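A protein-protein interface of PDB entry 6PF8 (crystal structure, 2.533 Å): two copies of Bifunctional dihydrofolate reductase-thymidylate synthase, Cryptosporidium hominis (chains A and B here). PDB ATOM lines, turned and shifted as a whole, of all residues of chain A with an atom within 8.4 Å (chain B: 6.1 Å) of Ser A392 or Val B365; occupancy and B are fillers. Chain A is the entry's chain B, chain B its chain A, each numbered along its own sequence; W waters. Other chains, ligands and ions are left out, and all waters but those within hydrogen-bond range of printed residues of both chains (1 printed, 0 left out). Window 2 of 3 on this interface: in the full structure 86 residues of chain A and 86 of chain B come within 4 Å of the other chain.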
ATOM      1  N   PRO A 340      10.336  -6.700 -14.167  1.00  0.00           N
ATOM      2  CA  PRO A 340      11.689  -7.192 -14.462  1.00  0.00           C
ATOM      3  C   PRO A 340      12.017  -8.380 -13.567  1.00  0.00           C
ATOM      4  O   PRO A 340      12.438  -8.216 -12.417  1.00  0.00           O
ATOM      5  CB  PRO A 340      12.570  -5.971 -14.159  1.00  0.00           C
ATOM      6  CG  PRO A 340      11.811  -5.241 -13.089  1.00  0.00           C
ATOM      7  CD  PRO A 340      10.350  -5.441 -13.401  1.00  0.00           C
ATOM      8  N   GLN A 345      16.584  -9.679 -16.015  1.00  0.00           N
ATOM      9  CA  GLN A 345      17.915  -9.583 -15.438  1.00  0.00           C
ATOM     10  C   GLN A 345      18.921 -10.417 -16.220  1.00  0.00           C
ATOM     11  O   GLN A 345      20.113 -10.092 -16.233  1.00  0.00           O
ATOM     12  CB  GLN A 345      17.879 -10.015 -13.970  1.00  0.00           C
ATOM     13  CG  GLN A 345      16.775  -9.349 -13.173  1.00  0.00           C
ATOM     14  CD  GLN A 345      16.887  -7.838 -13.161  1.00  0.00           C
ATOM     15  OE1 GLN A 345      17.983  -7.280 -13.243  1.00  0.00           O
ATOM     16  NE2 GLN A 345      15.745  -7.162 -13.063  1.00  0.00           N
ATOM     17  N   TYR A 349      20.236  -6.664 -17.453  1.00  0.00           N
ATOM     18  CA  TYR A 349      20.479  -6.413 -16.038  1.00  0.00           C
ATOM     19  C   TYR A 349      20.693  -4.925 -15.788  1.00  0.00           C
ATOM     20  O   TYR A 349      21.423  -4.254 -16.522  1.00  0.00           O
ATOM     21  CB  TYR A 349      21.689  -7.207 -15.545  1.00  0.00           C
ATOM     22  CG  TYR A 349      21.842  -7.153 -14.041  1.00  0.00           C
ATOM     23  CD1 TYR A 349      21.200  -8.078 -13.226  1.00  0.00           C
ATOM     24  CD2 TYR A 349      22.606  -6.164 -13.435  1.00  0.00           C
ATOM     25  CE1 TYR A 349      21.325  -8.025 -11.851  1.00  0.00           C
ATOM     26  CE2 TYR A 349      22.733  -6.101 -12.061  1.00  0.00           C
ATOM     27  CZ  TYR A 349      22.093  -7.035 -11.275  1.00  0.00           C
ATOM     28  OH  TYR A 349      22.219  -6.982  -9.908  1.00  0.00           O
ATOM     29  N   ASN A 350      20.051  -4.417 -14.736  1.00  0.00           N
ATOM     30  CA  ASN A 350      20.052  -3.010 -14.340  1.00  0.00           C
ATOM     31  C   ASN A 350      19.363  -2.104 -15.350  1.00  0.00           C
ATOM     32  O   ASN A 350      19.436  -0.876 -15.216  1.00  0.00           O
ATOM     33  CB  ASN A 350      21.471  -2.490 -14.078  1.00  0.00           C
ATOM     34  CG  ASN A 350      21.941  -2.772 -12.664  1.00  0.00           C
ATOM     35  OD1 ASN A 350      21.138  -2.833 -11.734  1.00  0.00           O
ATOM     36  ND2 ASN A 350      23.248  -2.945 -12.495  1.00  0.00           N
ATOM     37  N   GLY A 351      18.692  -2.662 -16.352  1.00  0.00           N
ATOM     38  CA  GLY A 351      17.962  -1.834 -17.294  1.00  0.00           C
ATOM     39  C   GLY A 351      16.694  -1.278 -16.669  1.00  0.00           C
ATOM     40  O   GLY A 351      16.017  -1.943 -15.884  1.00  0.00           O
ATOM     41  N   GLU A 352      16.377  -0.033 -17.018  1.00  0.00           N
ATOM     42  CA  GLU A 352      15.188   0.617 -16.482  1.00  0.00           C
ATOM     43  C   GLU A 352      13.936   0.012 -17.108  1.00  0.00           C
ATOM     44  O   GLU A 352      13.755   0.067 -18.328  1.00  0.00           O
ATOM     45  CB  GLU A 352      15.244   2.122 -16.732  1.00  0.00           C
ATOM     46  CG  GLU A 352      14.126   2.901 -16.051  1.00  0.00           C
ATOM     47  CD  GLU A 352      14.196   2.822 -14.533  1.00  0.00           C
ATOM     48  OE1 GLU A 352      15.318   2.708 -13.994  1.00  0.00           O
ATOM     49  OE2 GLU A 352      13.132   2.867 -13.878  1.00  0.00           O
ATOM     50  N   ALA A 388      20.245 -13.103 -10.891  1.00  0.00           N
ATOM     51  CA  ALA A 388      18.969 -12.427 -11.057  1.00  0.00           C
ATOM     52  C   ALA A 388      18.580 -11.577  -9.856  1.00  0.00           C
ATOM     53  O   ALA A 388      17.534 -10.921  -9.900  1.00  0.00           O
ATOM     54  CB  ALA A 388      17.849 -13.441 -11.335  1.00  0.00           C
ATOM     55  N   TRP A 389      19.377 -11.568  -8.791  1.00  0.00           N
ATOM     56  CA  TRP A 389      19.039 -10.807  -7.590  1.00  0.00           C
ATOM     57  C   TRP A 389      19.531  -9.377  -7.769  1.00  0.00           C
ATOM     58  O   TRP A 389      20.712  -9.082  -7.572  1.00  0.00           O
ATOM     59  CB  TRP A 389      19.641 -11.450  -6.346  1.00  0.00           C
ATOM     60  CG  TRP A 389      19.053 -10.906  -5.092  1.00  0.00           C
ATOM     61  CD1 TRP A 389      19.595  -9.961  -4.273  1.00  0.00           C
ATOM     62  CD2 TRP A 389      17.785 -11.250  -4.528  1.00  0.00           C
ATOM     63  NE1 TRP A 389      18.747  -9.705  -3.223  1.00  0.00           N
ATOM     64  CE2 TRP A 389      17.628 -10.484  -3.357  1.00  0.00           C
ATOM     65  CE3 TRP A 389      16.768 -12.137  -4.896  1.00  0.00           C
ATOM     66  CZ2 TRP A 389      16.496 -10.578  -2.550  1.00  0.00           C
ATOM     67  CZ3 TRP A 389      15.644 -12.227  -4.095  1.00  0.00           C
ATOM     68  CH2 TRP A 389      15.518 -11.453  -2.935  1.00  0.00           C
ATOM     69  N   ASN A 390      18.612  -8.483  -8.123  1.00  0.00           N
ATOM     70  CA  ASN A 390      18.911  -7.069  -8.328  1.00  0.00           C
ATOM     71  C   ASN A 390      18.184  -6.258  -7.267  1.00  0.00           C
ATOM     72  O   ASN A 390      16.970  -6.033  -7.385  1.00  0.00           O
ATOM     73  CB  ASN A 390      18.483  -6.627  -9.731  1.00  0.00           C
ATOM     74  CG  ASN A 390      19.034  -5.266 -10.113  1.00  0.00           C
ATOM     75  OD1 ASN A 390      19.343  -4.439  -9.255  1.00  0.00           O
ATOM     76  ND2 ASN A 390      19.144  -5.022 -11.414  1.00  0.00           N
ATOM     77  N   PRO A 391      18.874  -5.800  -6.216  1.00  0.00           N
ATOM     78  CA  PRO A 391      18.183  -5.042  -5.159  1.00  0.00           C
ATOM     79  C   PRO A 391      17.469  -3.798  -5.663  1.00  0.00           C
ATOM     80  O   PRO A 391      16.499  -3.356  -5.035  1.00  0.00           O
ATOM     81  CB  PRO A 391      19.318  -4.686  -4.190  1.00  0.00           C
ATOM     82  CG  PRO A 391      20.347  -5.752  -4.407  1.00  0.00           C
ATOM     83  CD  PRO A 391      20.276  -6.093  -5.872  1.00  0.00           C
ATOM     84  N   SER A 392      17.907  -3.224  -6.785  1.00  0.00           N
ATOM     85  CA  SER A 392      17.253  -2.026  -7.296  1.00  0.00           C
ATOM     86  C   SER A 392      15.909  -2.327  -7.945  1.00  0.00           C
ATOM     87  O   SER A 392      15.080  -1.420  -8.065  1.00  0.00           O
ATOM     88  CB  SER A 392      18.160  -1.310  -8.301  1.00  0.00           C
ATOM     89  OG  SER A 392      19.355  -0.860  -7.687  1.00  0.00           O
ATOM     90  N   ALA A 393      15.665  -3.572  -8.349  1.00  0.00           N
ATOM     91  CA  ALA A 393      14.462  -3.914  -9.095  1.00  0.00           C
ATOM     92  C   ALA A 393      13.492  -4.797  -8.321  1.00  0.00           C
ATOM     93  O   ALA A 393      12.406  -5.090  -8.833  1.00  0.00           O
ATOM     94  CB  ALA A 393      14.842  -4.599 -10.411  1.00  0.00           C
ATOM     95  N   LEU A 394      13.836  -5.204  -7.096  1.00  0.00           N
ATOM     96  CA  LEU A 394      13.003  -6.155  -6.362  1.00  0.00           C
ATOM     97  C   LEU A 394      11.586  -5.626  -6.163  1.00  0.00           C
ATOM     98  O   LEU A 394      10.613  -6.381  -6.274  1.00  0.00           O
ATOM     99  CB  LEU A 394      13.646  -6.474  -5.012  1.00  0.00           C
ATOM    100  CG  LEU A 394      15.001  -7.182  -5.038  1.00  0.00           C
ATOM    101  CD1 LEU A 394      15.555  -7.306  -3.629  1.00  0.00           C
ATOM    102  CD2 LEU A 394      14.887  -8.548  -5.694  1.00  0.00           C
ATOM    103  N   SER A 395      11.448  -4.328  -5.883  1.00  0.00           N
ATOM    104  CA  SER A 395      10.128  -3.768  -5.607  1.00  0.00           C
ATOM    105  C   SER A 395       9.227  -3.800  -6.836  1.00  0.00           C
ATOM    106  O   SER A 395       7.999  -3.815  -6.700  1.00  0.00           O
ATOM    107  CB  SER A 395      10.263  -2.336  -5.089  1.00  0.00           C
ATOM    108  OG  SER A 395      10.901  -1.516  -6.052  1.00  0.00           O
ATOM    109  N   GLN A 396       9.807  -3.807  -8.035  1.00  0.00           N
ATOM    110  CA  GLN A 396       9.026  -3.815  -9.264  1.00  0.00           C
ATOM    111  C   GLN A 396       8.640  -5.216  -9.718  1.00  0.00           C
ATOM    112  O   GLN A 396       7.825  -5.346 -10.638  1.00  0.00           O
ATOM    113  CB  GLN A 396       9.807  -3.127 -10.390  1.00  0.00           C
ATOM    114  CG  GLN A 396      10.250  -1.705 -10.083  1.00  0.00           C
ATOM    115  CD  GLN A 396      11.128  -1.126 -11.179  1.00  0.00           C
ATOM    116  OE1 GLN A 396      12.311  -0.862 -10.965  1.00  0.00           O
ATOM    117  NE2 GLN A 396      10.555  -0.931 -12.361  1.00  0.00           N
ATOM    118  N   MET A 397       9.196  -6.258  -9.104  1.00  0.00           N
ATOM    119  CA  MET A 397       8.947  -7.623  -9.549  1.00  0.00           C
ATOM    120  C   MET A 397       7.645  -8.160  -8.975  1.00  0.00           C
ATOM    121  O   MET A 397       7.308  -7.905  -7.816  1.00  0.00           O
ATOM    122  CB  MET A 397      10.098  -8.542  -9.141  1.00  0.00           C
ATOM    123  CG  MET A 397      11.454  -8.072  -9.609  1.00  0.00           C
ATOM    124  SD  MET A 397      12.759  -9.285  -9.327  1.00  0.00           S
ATOM    125  CE  MET A 397      14.223  -8.305  -9.668  1.00  0.00           C
ATOM    126  N   PHE B 344      31.103  -2.087  -0.626  1.00  0.00           N
ATOM    127  CA  PHE B 344      30.488  -1.018  -1.386  1.00  0.00           C
ATOM    128  C   PHE B 344      29.194  -1.486  -2.009  1.00  0.00           C
ATOM    129  O   PHE B 344      28.242  -0.712  -2.088  1.00  0.00           O
ATOM    130  CB  PHE B 344      31.430  -0.491  -2.482  1.00  0.00           C
ATOM    131  CG  PHE B 344      30.870   0.697  -3.240  1.00  0.00           C
ATOM    132  CD1 PHE B 344      31.153   1.988  -2.826  1.00  0.00           C
ATOM    133  CD2 PHE B 344      30.069   0.526  -4.367  1.00  0.00           C
ATOM    134  CE1 PHE B 344      30.647   3.079  -3.496  1.00  0.00           C
ATOM    135  CE2 PHE B 344      29.552   1.626  -5.043  1.00  0.00           C
ATOM    136  CZ  PHE B 344      29.848   2.902  -4.605  1.00  0.00           C
ATOM    137  N   GLN B 345      29.136  -2.757  -2.408  1.00  0.00           N
ATOM    138  CA  GLN B 345      27.868  -3.352  -2.796  1.00  0.00           C
ATOM    139  C   GLN B 345      26.998  -3.647  -1.582  1.00  0.00           C
ATOM    140  O   GLN B 345      25.768  -3.677  -1.700  1.00  0.00           O
ATOM    141  CB  GLN B 345      28.118  -4.631  -3.600  1.00  0.00           C
ATOM    142  CG  GLN B 345      29.136  -4.461  -4.716  1.00  0.00           C
ATOM    143  CD  GLN B 345      28.738  -3.415  -5.741  1.00  0.00           C
ATOM    144  OE1 GLN B 345      27.554  -3.191  -5.993  1.00  0.00           O
ATOM    145  NE2 GLN B 345      29.733  -2.752  -6.322  1.00  0.00           N
ATOM    146  N   TRP B 346      27.611  -3.870  -0.415  1.00  0.00           N
ATOM    147  CA  TRP B 346      26.833  -4.095   0.801  1.00  0.00           C
ATOM    148  C   TRP B 346      26.063  -2.845   1.204  1.00  0.00           C
ATOM    149  O   TRP B 346      24.895  -2.929   1.600  1.00  0.00           O
ATOM    150  CB  TRP B 346      27.737  -4.537   1.953  1.00  0.00           C
ATOM    151  CG  TRP B 346      28.287  -5.932   1.844  1.00  0.00           C
ATOM    152  CD1 TRP B 346      28.338  -6.716   0.727  1.00  0.00           C
ATOM    153  CD2 TRP B 346      28.844  -6.716   2.908  1.00  0.00           C
ATOM    154  NE1 TRP B 346      28.908  -7.931   1.027  1.00  0.00           N
ATOM    155  CE2 TRP B 346      29.224  -7.957   2.360  1.00  0.00           C
ATOM    156  CE3 TRP B 346      29.063  -6.486   4.271  1.00  0.00           C
ATOM    157  CZ2 TRP B 346      29.810  -8.964   3.125  1.00  0.00           C
ATOM    158  CZ3 TRP B 346      29.644  -7.485   5.028  1.00  0.00           C
ATOM    159  CH2 TRP B 346      30.011  -8.708   4.454  1.00  0.00           C
ATOM    160  N   ARG B 347      26.703  -1.676   1.120  1.00  0.00           N
ATOM    161  CA  ARG B 347      26.123  -0.438   1.619  1.00  0.00           C
ATOM    162  C   ARG B 347      25.661   0.521   0.529  1.00  0.00           C
ATOM    163  O   ARG B 347      24.830   1.389   0.812  1.00  0.00           O
ATOM    164  CB  ARG B 347      27.129   0.290   2.525  1.00  0.00           C
ATOM    165  CG  ARG B 347      27.807  -0.615   3.547  1.00  0.00           C
ATOM    166  CD  ARG B 347      26.796  -1.378   4.390  1.00  0.00           C
ATOM    167  NE  ARG B 347      25.816  -0.495   5.011  1.00  0.00           N
ATOM    168  CZ  ARG B 347      26.037   0.184   6.133  1.00  0.00           C
ATOM    169  NH1 ARG B 347      27.206   0.081   6.750  1.00  0.00           N
ATOM    170  NH2 ARG B 347      25.092   0.966   6.636  1.00  0.00           N
ATOM    171  N   HIS B 348      26.180   0.402  -0.695  1.00  0.00           N
ATOM    172  CA  HIS B 348      25.837   1.316  -1.783  1.00  0.00           C
ATOM    173  C   HIS B 348      25.699   0.538  -3.095  1.00  0.00           C
ATOM    174  O   HIS B 348      26.391   0.796  -4.077  1.00  0.00           O
ATOM    175  CB  HIS B 348      26.883   2.421  -1.934  1.00  0.00           C
ATOM    176  CG  HIS B 348      27.325   3.026  -0.638  1.00  0.00           C
ATOM    177  ND1 HIS B 348      26.530   3.881   0.095  1.00  0.00           N
ATOM    178  CD2 HIS B 348      28.483   2.902   0.053  1.00  0.00           C
ATOM    179  CE1 HIS B 348      27.179   4.255   1.183  1.00  0.00           C
ATOM    180  NE2 HIS B 348      28.366   3.676   1.182  1.00  0.00           N
ATOM    181  N   TYR B 349      24.798  -0.442  -3.119  1.00  0.00           N
ATOM    182  CA  TYR B 349      24.629  -1.255  -4.316  1.00  0.00           C
ATOM    183  C   TYR B 349      24.102  -0.407  -5.469  1.00  0.00           C
ATOM    184  O   TYR B 349      23.177   0.393  -5.302  1.00  0.00           O
ATOM    185  CB  TYR B 349      23.685  -2.426  -4.052  1.00  0.00           C
ATOM    186  CG  TYR B 349      23.681  -3.431  -5.182  1.00  0.00           C
ATOM    187  CD1 TYR B 349      24.594  -4.478  -5.202  1.00  0.00           C
ATOM    188  CD2 TYR B 349      22.785  -3.321  -6.240  1.00  0.00           C
ATOM    189  CE1 TYR B 349      24.607  -5.392  -6.233  1.00  0.00           C
ATOM    190  CE2 TYR B 349      22.794  -4.230  -7.279  1.00  0.00           C
ATOM    191  CZ  TYR B 349      23.707  -5.265  -7.267  1.00  0.00           C
ATOM    192  OH  TYR B 349      23.723  -6.180  -8.295  1.00  0.00           O
ATOM    193  N   ASN B 350      24.699  -0.593  -6.648  1.00  0.00           N
ATOM    194  CA  ASN B 350      24.412   0.152  -7.872  1.00  0.00           C
ATOM    195  C   ASN B 350      24.786   1.625  -7.772  1.00  0.00           C
ATOM    196  O   ASN B 350      24.445   2.404  -8.669  1.00  0.00           O
ATOM    197  CB  ASN B 350      22.942   0.035  -8.292  1.00  0.00           C
ATOM    198  CG  ASN B 350      22.669  -1.207  -9.107  1.00  0.00           C
ATOM    199  OD1 ASN B 350      23.548  -1.703  -9.812  1.00  0.00           O
ATOM    200  ND2 ASN B 350      21.444  -1.713  -9.028  1.00  0.00           N
ATOM    201  N   GLY B 351      25.468   2.033  -6.706  1.00  0.00           N
ATOM    202  CA  GLY B 351      25.919   3.410  -6.606  1.00  0.00           C
ATOM    203  C   GLY B 351      27.098   3.669  -7.528  1.00  0.00           C
ATOM    204  O   GLY B 351      27.956   2.809  -7.729  1.00  0.00           O
ATOM    205  N   VAL B 363      24.032   7.295  -1.516  1.00  0.00           N
ATOM    206  CA  VAL B 363      24.028   6.727  -2.860  1.00  0.00           C
ATOM    207  C   VAL B 363      23.925   5.210  -2.770  1.00  0.00           C
ATOM    208  O   VAL B 363      24.454   4.584  -1.841  1.00  0.00           O
ATOM    209  CB  VAL B 363      25.276   7.168  -3.654  1.00  0.00           C
ATOM    210  CG1 VAL B 363      26.529   6.468  -3.151  1.00  0.00           C
ATOM    211  CG2 VAL B 363      25.082   6.917  -5.141  1.00  0.00           C
ATOM    212  N   GLY B 364      23.219   4.615  -3.729  1.00  0.00           N
ATOM    213  CA  GLY B 364      23.075   3.177  -3.796  1.00  0.00           C
ATOM    214  C   GLY B 364      22.101   2.625  -2.769  1.00  0.00           C
ATOM    215  O   GLY B 364      21.584   3.326  -1.898  1.00  0.00           O
ATOM    216  N   VAL B 365      21.851   1.321  -2.884  1.00  0.00           N
ATOM    217  CA  VAL B 365      20.952   0.611  -1.982  1.00  0.00           C
ATOM    218  C   VAL B 365      21.754   0.069  -0.806  1.00  0.00           C
ATOM    219  O   VAL B 365      22.750  -0.640  -0.996  1.00  0.00           O
ATOM    220  CB  VAL B 365      20.219  -0.523  -2.718  1.00  0.00           C
ATOM    221  CG1 VAL B 365      19.254  -1.227  -1.775  1.00  0.00           C
ATOM    222  CG2 VAL B 365      19.490   0.021  -3.939  1.00  0.00           C
ATOM    223  N   ASP B 366      21.317   0.393   0.410  1.00  0.00           N
ATOM    224  CA  ASP B 366      21.980  -0.078   1.626  1.00  0.00           C
ATOM    225  C   ASP B 366      21.412  -1.449   1.966  1.00  0.00           C
ATOM    226  O   ASP B 366      20.427  -1.574   2.695  1.00  0.00           O
ATOM    227  CB  ASP B 366      21.788   0.914   2.766  1.00  0.00           C
ATOM    228  CG  ASP B 366      22.785   0.712   3.894  1.00  0.00           C
ATOM    229  OD1 ASP B 366      23.320  -0.409   4.026  1.00  0.00           O
ATOM    230  OD2 ASP B 366      23.030   1.673   4.654  1.00  0.00           O
ATOM    231  N   GLN B 367      22.044  -2.496   1.425  1.00  0.00           N
ATOM    232  CA  GLN B 367      21.565  -3.856   1.658  1.00  0.00           C
ATOM    233  C   GLN B 367      21.662  -4.243   3.127  1.00  0.00           C
ATOM    234  O   GLN B 367      20.738  -4.857   3.676  1.00  0.00           O
ATOM    235  CB  GLN B 367      22.358  -4.851   0.811  1.00  0.00           C
ATOM    236  CG  GLN B 367      22.114  -4.789  -0.680  1.00  0.00           C
ATOM    237  CD  GLN B 367      22.827  -5.915  -1.403  1.00  0.00           C
ATOM    238  OE1 GLN B 367      22.301  -7.023  -1.524  1.00  0.00           O
ATOM    239  NE2 GLN B 367      24.037  -5.642  -1.874  1.00  0.00           N
ATOM    240  N   LEU B 368      22.783  -3.912   3.774  1.00  0.00           N
ATOM    241  CA  LEU B 368      22.992  -4.327   5.157  1.00  0.00           C
ATOM    242  C   LEU B 368      21.954  -3.707   6.086  1.00  0.00           C
ATOM    243  O   LEU B 368      21.420  -4.385   6.972  1.00  0.00           O
ATOM    244  CB  LEU B 368      24.407  -3.957   5.601  1.00  0.00           C
ATOM    245  CG  LEU B 368      24.859  -4.481   6.965  1.00  0.00           C
ATOM    246  CD1 LEU B 368      24.733  -5.997   7.027  1.00  0.00           C
ATOM    247  CD2 LEU B 368      26.289  -4.046   7.260  1.00  0.00           C
ATOM    248  N   LYS B 370      18.900  -2.667   5.255  1.00  0.00           N
ATOM    249  CA  LYS B 370      17.605  -3.282   4.984  1.00  0.00           C
ATOM    250  C   LYS B 370      17.551  -4.717   5.492  1.00  0.00           C
ATOM    251  O   LYS B 370      16.495  -5.170   5.948  1.00  0.00           O
ATOM    252  CB  LYS B 370      17.295  -3.225   3.486  1.00  0.00           C
ATOM    253  CG  LYS B 370      17.316  -1.808   2.922  1.00  0.00           C
ATOM    254  CD  LYS B 370      16.829  -1.743   1.482  1.00  0.00           C
ATOM    255  CE  LYS B 370      15.318  -1.600   1.415  1.00  0.00           C
ATOM    256  NZ  LYS B 370      14.850  -1.352   0.024  1.00  0.00           N
HETATM  257  O   HOH W   1      19.499  -7.815  -1.109  1.00  0.00           O
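Printed residues of chain B within 4 Å of Asn A350: Asn B350. Of the printed residues of chain B, Asn A390 touches Tyr B349 and Asn B350. Of chain B, only Asn B350 (2.6 Å) and Val B365 (3.9 Å) come within 4 Å of Ser A392. Of the printed residues of chain A, Tyr B349 touches Tyr A349, Asn A390 and Pro A391. No residue of chain A comes within 4 Å of Gly B364. Of chain A, only Ser A392 comes within 4 Å of Val B365. Of the printed residues of chain A, Gln B367 touches Pro A391. The nearest residue of chain A that does not touch Val B365 is Pro A391 (4.2 Å).
Among the printed residues, merely in contact across the chains: Pro A391 with Tyr B349 (3.4 Å), Pro A391 with Gln B367 (3.7 Å), Ser A392 with Val B365 (3.9 Å) and Asn A390 with Tyr B349 (3.98 Å).
O of Trp B346 sits at hydrogen-bond distance from N of Gln B367, 2.9 Å away. The side-chain amide nitrogen of Gln B367 sits at hydrogen-bond distance from the backbone carbonyl oxygen of Gln B345. O of Tyr B349 sits at hydrogen-bond distance from N of Val B365 (2.9 Å). The side-chain amide oxygen of Gln A345 lies within hydrogen-bond range of the side-chain amide nitrogen of Asn A390, at 3.1 Å. The side-chain amide oxygen (OD1) of Asn A350 sits at hydrogen-bond distance from the side-chain amide nitrogen (ND2) of Asn A390, at 3.0 Å. N of Ser A392 lies close to OD1 of Asn A390, 3.1 Å away.
The side-chain amide oxygen (OD1) of Asn A350 is in hydrogen-bond range of the side-chain amide nitrogen (ND2) of Asn B350 (2.9 Å). The side-chain amide nitrogen of Asn B350 is in hydrogen-bond range of the side-chain amide oxygen of Asn A390, 3.4 Å away. The side-chain amide nitrogen (ND2) of Asn B350 sits at hydrogen-bond distance from the side-chain hydroxyl (OG) of Ser A392 (2.6 Å). The side-chain hydroxyl of Tyr A349 sits close to the side-chain hydroxyl of Tyr B349 (2.3 Å).
Tyr A349 touches its own counterpart, Tyr B349. Asn A350 touches its own counterpart, Asn B350. 4 positions are printed for both chains. Of the 8 pairs that touch across the chains among the printed residues, 2 have their exchanged pair printed and touching as well.
Of the 15 printed residues of chain B, 4 touch a printed residue of chain A. Printed residues of chain B that touch a printed residue of chain A: Tyr B349, Asn B350, Val B365 and Gln B367. Hydrophobic or aromatic side chains of chain B that line the printed part of chain A: Tyr B349 and Val B365. Along chain B the printed residues that touch a printed residue of chain A span positions 349 to 367. Of the 16 printed residues of chain A, 5 touch a printed residue of chain B. Among the printed residues, 8 pairs touch across the chains. Among the printed residues, no Asp or Glu carboxylate lies within 4 Å of a Lys or Arg side-chain nitrogen of the other chain.
Water W1 lies within hydrogen-bond range of the indole nitrogen of Trp A389 and the side-chain amide oxygen of Gln B367.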
